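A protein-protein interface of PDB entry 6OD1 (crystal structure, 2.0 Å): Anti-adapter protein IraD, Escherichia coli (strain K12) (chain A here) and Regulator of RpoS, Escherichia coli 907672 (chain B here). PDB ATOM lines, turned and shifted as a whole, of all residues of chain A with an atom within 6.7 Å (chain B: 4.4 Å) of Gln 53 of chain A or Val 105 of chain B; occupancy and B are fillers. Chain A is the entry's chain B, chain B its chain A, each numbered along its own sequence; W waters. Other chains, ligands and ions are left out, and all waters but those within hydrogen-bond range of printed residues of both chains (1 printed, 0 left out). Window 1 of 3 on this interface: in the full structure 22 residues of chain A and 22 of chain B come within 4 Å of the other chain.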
ATOM      1  N   PRO A  26      -4.212  33.141 -22.416  1.00  0.00           N
ATOM      2  CA  PRO A  26      -4.262  33.064 -23.881  1.00  0.00           C
ATOM      3  C   PRO A  26      -5.570  33.609 -24.462  1.00  0.00           C
ATOM      4  O   PRO A  26      -6.668  33.356 -23.957  1.00  0.00           O
ATOM      5  CB  PRO A  26      -4.094  31.568 -24.152  1.00  0.00           C
ATOM      6  CG  PRO A  26      -3.250  31.075 -22.957  1.00  0.00           C
ATOM      7  CD  PRO A  26      -3.737  31.887 -21.791  1.00  0.00           C
ATOM      8  N   LEU A  28      -7.012  32.716 -27.065  1.00  0.00           N
ATOM      9  CA  LEU A  28      -7.815  31.557 -27.443  1.00  0.00           C
ATOM     10  C   LEU A  28      -8.894  31.243 -26.405  1.00  0.00           C
ATOM     11  O   LEU A  28     -10.030  30.893 -26.762  1.00  0.00           O
ATOM     12  CB  LEU A  28      -6.887  30.353 -27.629  1.00  0.00           C
ATOM     13  CG  LEU A  28      -7.365  29.130 -28.404  1.00  0.00           C
ATOM     14  CD1 LEU A  28      -7.764  29.509 -29.802  1.00  0.00           C
ATOM     15  CD2 LEU A  28      -6.262  28.070 -28.427  1.00  0.00           C
ATOM     16  N   LEU A  29      -8.561  31.382 -25.119  1.00  0.00           N
ATOM     17  CA  LEU A  29      -9.448  30.989 -24.032  1.00  0.00           C
ATOM     18  C   LEU A  29     -10.367  32.099 -23.563  1.00  0.00           C
ATOM     19  O   LEU A  29     -11.417  31.801 -22.979  1.00  0.00           O
ATOM     20  CB  LEU A  29      -8.641  30.524 -22.823  1.00  0.00           C
ATOM     21  CG  LEU A  29      -7.617  29.438 -23.098  1.00  0.00           C
ATOM     22  CD1 LEU A  29      -6.925  29.065 -21.813  1.00  0.00           C
ATOM     23  CD2 LEU A  29      -8.291  28.243 -23.732  1.00  0.00           C
ATOM     24  N   SER A  48     -14.691  19.845 -23.316  1.00  0.00           N
ATOM     25  CA  SER A  48     -13.796  19.278 -22.310  1.00  0.00           C
ATOM     26  C   SER A  48     -12.381  19.805 -22.494  1.00  0.00           C
ATOM     27  O   SER A  48     -11.698  20.113 -21.511  1.00  0.00           O
ATOM     28  CB  SER A  48     -13.828  17.748 -22.372  1.00  0.00           C
ATOM     29  OG  SER A  48     -12.933  17.248 -23.354  1.00  0.00           O
ATOM     30  N   TRP A  49     -11.937  19.951 -23.752  1.00  0.00           N
ATOM     31  CA  TRP A  49     -10.647  20.587 -24.016  1.00  0.00           C
ATOM     32  C   TRP A  49     -10.590  21.982 -23.407  1.00  0.00           C
ATOM     33  O   TRP A  49      -9.604  22.345 -22.761  1.00  0.00           O
ATOM     34  CB  TRP A  49     -10.360  20.674 -25.522  1.00  0.00           C
ATOM     35  CG  TRP A  49      -9.158  21.592 -25.831  1.00  0.00           C
ATOM     36  CD1 TRP A  49      -7.821  21.232 -25.864  1.00  0.00           C
ATOM     37  CD2 TRP A  49      -9.193  23.002 -26.115  1.00  0.00           C
ATOM     38  NE1 TRP A  49      -7.044  22.334 -26.163  1.00  0.00           N
ATOM     39  CE2 TRP A  49      -7.864  23.427 -26.320  1.00  0.00           C
ATOM     40  CE3 TRP A  49     -10.229  23.944 -26.243  1.00  0.00           C
ATOM     41  CZ2 TRP A  49      -7.541  24.749 -26.637  1.00  0.00           C
ATOM     42  CZ3 TRP A  49      -9.902  25.266 -26.548  1.00  0.00           C
ATOM     43  CH2 TRP A  49      -8.567  25.653 -26.737  1.00  0.00           C
ATOM     44  N   TYR A  50     -11.627  22.788 -23.626  1.00  0.00           N
ATOM     45  CA  TYR A  50     -11.595  24.170 -23.145  1.00  0.00           C
ATOM     46  C   TYR A  50     -11.418  24.215 -21.628  1.00  0.00           C
ATOM     47  O   TYR A  50     -10.584  24.962 -21.107  1.00  0.00           O
ATOM     48  CB  TYR A  50     -12.882  24.891 -23.562  1.00  0.00           C
ATOM     49  CG  TYR A  50     -12.953  26.335 -23.095  1.00  0.00           C
ATOM     50  CD1 TYR A  50     -13.827  26.712 -22.086  1.00  0.00           C
ATOM     51  CD2 TYR A  50     -12.136  27.321 -23.658  1.00  0.00           C
ATOM     52  CE1 TYR A  50     -13.902  28.024 -21.657  1.00  0.00           C
ATOM     53  CE2 TYR A  50     -12.192  28.633 -23.227  1.00  0.00           C
ATOM     54  CZ  TYR A  50     -13.091  28.986 -22.234  1.00  0.00           C
ATOM     55  OH  TYR A  50     -13.180  30.300 -21.799  1.00  0.00           O
ATOM     56  N   CYS A  51     -12.197  23.405 -20.903  1.00  0.00           N
ATOM     57  CA  CYS A  51     -12.105  23.393 -19.447  1.00  0.00           C
ATOM     58  C   CYS A  51     -10.734  22.947 -18.981  1.00  0.00           C
ATOM     59  O   CYS A  51     -10.190  23.511 -18.021  1.00  0.00           O
ATOM     60  CB  CYS A  51     -13.190  22.497 -18.852  1.00  0.00           C
ATOM     61  SG  CYS A  51     -14.902  23.057 -19.230  1.00  0.00           S
ATOM     62  N   ARG A  52     -10.147  21.968 -19.674  1.00  0.00           N
ATOM     63  CA  ARG A  52      -8.822  21.480 -19.301  1.00  0.00           C
ATOM     64  C   ARG A  52      -7.785  22.593 -19.399  1.00  0.00           C
ATOM     65  O   ARG A  52      -7.049  22.851 -18.445  1.00  0.00           O
ATOM     66  CB  ARG A  52      -8.428  20.297 -20.184  1.00  0.00           C
ATOM     67  CG  ARG A  52      -8.802  18.946 -19.619  1.00  0.00           C
ATOM     68  CD  ARG A  52      -7.964  17.836 -20.267  1.00  0.00           C
ATOM     69  NE  ARG A  52      -7.887  17.932 -21.733  1.00  0.00           N
ATOM     70  CZ  ARG A  52      -8.877  17.634 -22.563  1.00  0.00           C
ATOM     71  NH1 ARG A  52     -10.062  17.239 -22.087  1.00  0.00           N
ATOM     72  NH2 ARG A  52      -8.700  17.741 -23.878  1.00  0.00           N
ATOM     73  N   GLN A  53      -7.752  23.307 -20.529  1.00  0.00           N
ATOM     74  CA  GLN A  53      -6.692  24.299 -20.710  1.00  0.00           C
ATOM     75  C   GLN A  53      -6.958  25.571 -19.931  1.00  0.00           C
ATOM     76  O   GLN A  53      -6.009  26.238 -19.511  1.00  0.00           O
ATOM     77  CB  GLN A  53      -6.515  24.669 -22.185  1.00  0.00           C
ATOM     78  CG  GLN A  53      -6.337  23.517 -23.152  1.00  0.00           C
ATOM     79  CD  GLN A  53      -5.626  22.325 -22.548  1.00  0.00           C
ATOM     80  OE1 GLN A  53      -4.586  22.458 -21.882  1.00  0.00           O
ATOM     81  NE2 GLN A  53      -6.170  21.138 -22.798  1.00  0.00           N
ATOM     82  N   LEU A  54      -8.226  25.945 -19.762  1.00  0.00           N
ATOM     83  CA  LEU A  54      -8.520  27.108 -18.937  1.00  0.00           C
ATOM     84  C   LEU A  54      -8.105  26.855 -17.496  1.00  0.00           C
ATOM     85  O   LEU A  54      -7.477  27.710 -16.855  1.00  0.00           O
ATOM     86  CB  LEU A  54     -10.011  27.457 -19.041  1.00  0.00           C
ATOM     87  CG  LEU A  54     -10.443  28.676 -18.232  1.00  0.00           C
ATOM     88  CD1 LEU A  54      -9.620  29.892 -18.657  1.00  0.00           C
ATOM     89  CD2 LEU A  54     -11.924  28.928 -18.404  1.00  0.00           C
ATOM     90  N   ARG A  55      -8.393  25.662 -16.984  1.00  0.00           N
ATOM     91  CA  ARG A  55      -7.922  25.311 -15.655  1.00  0.00           C
ATOM     92  C   ARG A  55      -6.398  25.401 -15.557  1.00  0.00           C
ATOM     93  O   ARG A  55      -5.863  25.979 -14.607  1.00  0.00           O
ATOM     94  CB  ARG A  55      -8.415  23.916 -15.288  1.00  0.00           C
ATOM     95  CG  ARG A  55      -7.894  23.443 -13.970  1.00  0.00           C
ATOM     96  CD  ARG A  55      -8.250  21.990 -13.704  1.00  0.00           C
ATOM     97  NE  ARG A  55      -7.543  21.539 -12.512  1.00  0.00           N
ATOM     98  CZ  ARG A  55      -6.312  21.039 -12.505  1.00  0.00           C
ATOM     99  NH1 ARG A  55      -5.628  20.893 -13.645  1.00  0.00           N
ATOM    100  NH2 ARG A  55      -5.778  20.675 -11.352  1.00  0.00           N
ATOM    101  N   SER A  56      -5.677  24.846 -16.538  1.00  0.00           N
ATOM    102  CA  SER A  56      -4.221  24.933 -16.502  1.00  0.00           C
ATOM    103  C   SER A  56      -3.734  26.379 -16.554  1.00  0.00           C
ATOM    104  O   SER A  56      -2.794  26.750 -15.839  1.00  0.00           O
ATOM    105  CB  SER A  56      -3.612  24.129 -17.650  1.00  0.00           C
ATOM    106  OG  SER A  56      -3.923  22.758 -17.511  1.00  0.00           O
ATOM    107  N   ALA A  57      -4.335  27.200 -17.402  1.00  0.00           N
ATOM    108  CA  ALA A  57      -3.885  28.582 -17.536  1.00  0.00           C
ATOM    109  C   ALA A  57      -4.097  29.376 -16.245  1.00  0.00           C
ATOM    110  O   ALA A  57      -3.201  30.107 -15.816  1.00  0.00           O
ATOM    111  CB  ALA A  57      -4.601  29.235 -18.724  1.00  0.00           C
ATOM    112  N   LEU A  58      -5.275  29.244 -15.613  1.00  0.00           N
ATOM    113  CA  LEU A  58      -5.536  29.927 -14.343  1.00  0.00           C
ATOM    114  C   LEU A  58      -4.588  29.474 -13.236  1.00  0.00           C
ATOM    115  O   LEU A  58      -4.099  30.303 -12.449  1.00  0.00           O
ATOM    116  CB  LEU A  58      -6.986  29.696 -13.922  1.00  0.00           C
ATOM    117  CG  LEU A  58      -7.985  30.427 -14.824  1.00  0.00           C
ATOM    118  CD1 LEU A  58      -9.416  30.049 -14.485  1.00  0.00           C
ATOM    119  CD2 LEU A  58      -7.775  31.925 -14.706  1.00  0.00           C
ATOM    120  N   VAL B  84       0.118  17.908 -28.940  1.00  0.00           N
ATOM    121  CA  VAL B  84       0.390  19.196 -29.569  1.00  0.00           C
ATOM    122  C   VAL B  84       0.580  20.235 -28.481  1.00  0.00           C
ATOM    123  O   VAL B  84      -0.213  20.292 -27.535  1.00  0.00           O
ATOM    124  CB  VAL B  84      -0.752  19.598 -30.509  1.00  0.00           C
ATOM    125  CG1 VAL B  84      -0.416  20.921 -31.234  1.00  0.00           C
ATOM    126  CG2 VAL B  84      -1.025  18.461 -31.478  1.00  0.00           C
ATOM    127  N   ILE B  94      -7.499  24.303 -33.155  1.00  0.00           N
ATOM    128  CA  ILE B  94      -7.817  23.389 -32.062  1.00  0.00           C
ATOM    129  C   ILE B  94      -8.816  22.339 -32.534  1.00  0.00           C
ATOM    130  O   ILE B  94      -8.602  21.126 -32.379  1.00  0.00           O
ATOM    131  CB  ILE B  94      -8.367  24.180 -30.860  1.00  0.00           C
ATOM    132  CG1 ILE B  94      -7.357  25.245 -30.396  1.00  0.00           C
ATOM    133  CG2 ILE B  94      -8.823  23.222 -29.757  1.00  0.00           C
ATOM    134  CD1 ILE B  94      -5.911  24.694 -30.190  1.00  0.00           C
ATOM    135  N   ALA B  97      -7.256  19.788 -34.839  1.00  0.00           N
ATOM    136  CA  ALA B  97      -6.407  18.805 -34.183  1.00  0.00           C
ATOM    137  C   ALA B  97      -7.242  17.761 -33.449  1.00  0.00           C
ATOM    138  O   ALA B  97      -6.918  16.567 -33.477  1.00  0.00           O
ATOM    139  CB  ALA B  97      -5.444  19.504 -33.222  1.00  0.00           C
ATOM    140  N   VAL B 102      -5.758  13.555 -31.247  1.00  0.00           N
ATOM    141  CA  VAL B 102      -4.556  13.881 -30.485  1.00  0.00           C
ATOM    142  C   VAL B 102      -4.763  13.455 -29.038  1.00  0.00           C
ATOM    143  O   VAL B 102      -5.892  13.246 -28.583  1.00  0.00           O
ATOM    144  CB  VAL B 102      -4.201  15.387 -30.527  1.00  0.00           C
ATOM    145  CG1 VAL B 102      -3.772  15.808 -31.934  1.00  0.00           C
ATOM    146  CG2 VAL B 102      -5.389  16.215 -30.058  1.00  0.00           C
ATOM    147  N   ASP B 104      -3.888  15.582 -26.670  1.00  0.00           N
ATOM    148  CA  ASP B 104      -4.396  16.887 -26.248  1.00  0.00           C
ATOM    149  C   ASP B 104      -3.700  17.939 -27.104  1.00  0.00           C
ATOM    150  O   ASP B 104      -2.755  17.644 -27.840  1.00  0.00           O
ATOM    151  CB  ASP B 104      -4.155  17.164 -24.752  1.00  0.00           C
ATOM    152  CG  ASP B 104      -5.253  18.039 -24.137  1.00  0.00           C
ATOM    153  OD1 ASP B 104      -6.042  18.614 -24.913  1.00  0.00           O
ATOM    154  OD2 ASP B 104      -5.321  18.162 -22.893  1.00  0.00           O
ATOM    155  N   VAL B 105      -4.203  19.165 -27.028  1.00  0.00           N
ATOM    156  CA  VAL B 105      -3.506  20.342 -27.532  1.00  0.00           C
ATOM    157  C   VAL B 105      -3.254  21.211 -26.306  1.00  0.00           C
ATOM    158  O   VAL B 105      -4.197  21.762 -25.729  1.00  0.00           O
ATOM    159  CB  VAL B 105      -4.316  21.091 -28.596  1.00  0.00           C
ATOM    160  CG1 VAL B 105      -3.463  22.159 -29.310  1.00  0.00           C
ATOM    161  CG2 VAL B 105      -4.905  20.115 -29.638  1.00  0.00           C
ATOM    162  N   LEU B 106      -2.000  21.289 -25.872  1.00  0.00           N
ATOM    163  CA  LEU B 106      -1.610  22.131 -24.745  1.00  0.00           C
ATOM    164  C   LEU B 106      -1.233  23.524 -25.247  1.00  0.00           C
ATOM    165  O   LEU B 106      -0.798  23.693 -26.388  1.00  0.00           O
ATOM    166  CB  LEU B 106      -0.435  21.497 -23.986  1.00  0.00           C
ATOM    167  CG  LEU B 106      -0.734  20.569 -22.805  1.00  0.00           C
ATOM    168  CD1 LEU B 106      -1.880  19.668 -23.063  1.00  0.00           C
ATOM    169  CD2 LEU B 106       0.521  19.736 -22.323  1.00  0.00           C
ATOM    170  N   LEU B 107      -1.411  24.529 -24.398  1.00  0.00           N
ATOM    171  CA  LEU B 107      -1.116  25.901 -24.803  1.00  0.00           C
ATOM    172  C   LEU B 107       0.161  26.378 -24.120  1.00  0.00           C
ATOM    173  O   LEU B 107       0.464  25.986 -22.992  1.00  0.00           O
ATOM    174  CB  LEU B 107      -2.281  26.849 -24.480  1.00  0.00           C
ATOM    175  CG  LEU B 107      -3.689  26.531 -24.986  1.00  0.00           C
ATOM    176  CD1 LEU B 107      -4.660  27.657 -24.598  1.00  0.00           C
ATOM    177  CD2 LEU B 107      -3.723  26.339 -26.510  1.00  0.00           C
HETATM  178  O   HOH W   1      -2.678  24.148 -21.942  1.00  0.00           O
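Water W1 bridges OE1 of Gln 53 of chain A and N of Leu 107 of chain B.
Printed residues of chain A that touch a printed residue of chain B: Pro 26, Leu 28, Leu 29, Trp 49, Arg 52 and Gln 53.
Hydrophobic or aromatic side chains of chain A within 4 Å of the printed part of chain B: Pro 26, Leu 28, Leu 29 and Trp 49.
Among the printed residues, merely in contact across the chains: Pro 26 of chain A with Leu 107 of chain B (3.98 Å), Leu 28 of chain A with Ile 94 of chain B (3.6 Å), Leu 28 of chain A with Leu 107 of chain B (3.6 Å), Leu 29 of chain A with Leu 107 of chain B (3.8 Å), Trp 49 of chain A with Ile 94 of chain B (3.6 Å), Trp 49 of chain A with Asp 104 of chain B (3.3 Å) and Gln 53 of chain A with Val 105 of chain B (3.5 Å).
OD2 of Asp 104 of chain B lies within salt-bridge range of NE of Arg 52 of chain A.
The side-chain amide nitrogen of Gln 53 of chain A sits at hydrogen-bond distance from the side-chain carboxylate of Asp 104 of chain B.
The backbone carbonyl oxygen (O) of Val 105 of chain B is in hydrogen-bond range of the indole nitrogen (NE1) of Trp 49 of chain A (2.9 Å).
Of the printed residues of chain B, Gln 53 of chain A touches Asp 104 (3.1 Å) and Val 105 (3.5 Å).
Val 105 of chain B touches two residues of chain A.
Of the printed residues of chain A, Leu 107 of chain B touches Pro 26 (3.98 Å), Leu 28 (3.6 Å) and Leu 29 (3.8 Å).
Printed residues of chain B within 4 Å of Trp 49 of chain A: Ile 94, Asp 104 and Val 105.
Of the printed residues of chain B, Leu 28 of chain A touches Ile 94 (3.6 Å) and Leu 107 (3.6 Å).
Ser 56 of chain A touches none of the printed residues of chain B.
The backbone NH (N) of Val 84 of chain B is in hydrogen-bond range of the backbone carbonyl oxygen (O) of Asp 104 of chain B (3.1 Å).
OH of Tyr 50 of chain A lies within hydrogen-bond range of O of Leu 29 of chain A, at 2.6 Å.
The side-chain hydroxyl of Ser 48 of chain A lies within hydrogen-bond range of the guanidinium group of Arg 52 of chain A, 3.1 Å away.
O of Arg 52 of chain A sits at hydrogen-bond distance from OG of Ser 56 of chain A, 3.3 Å away.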
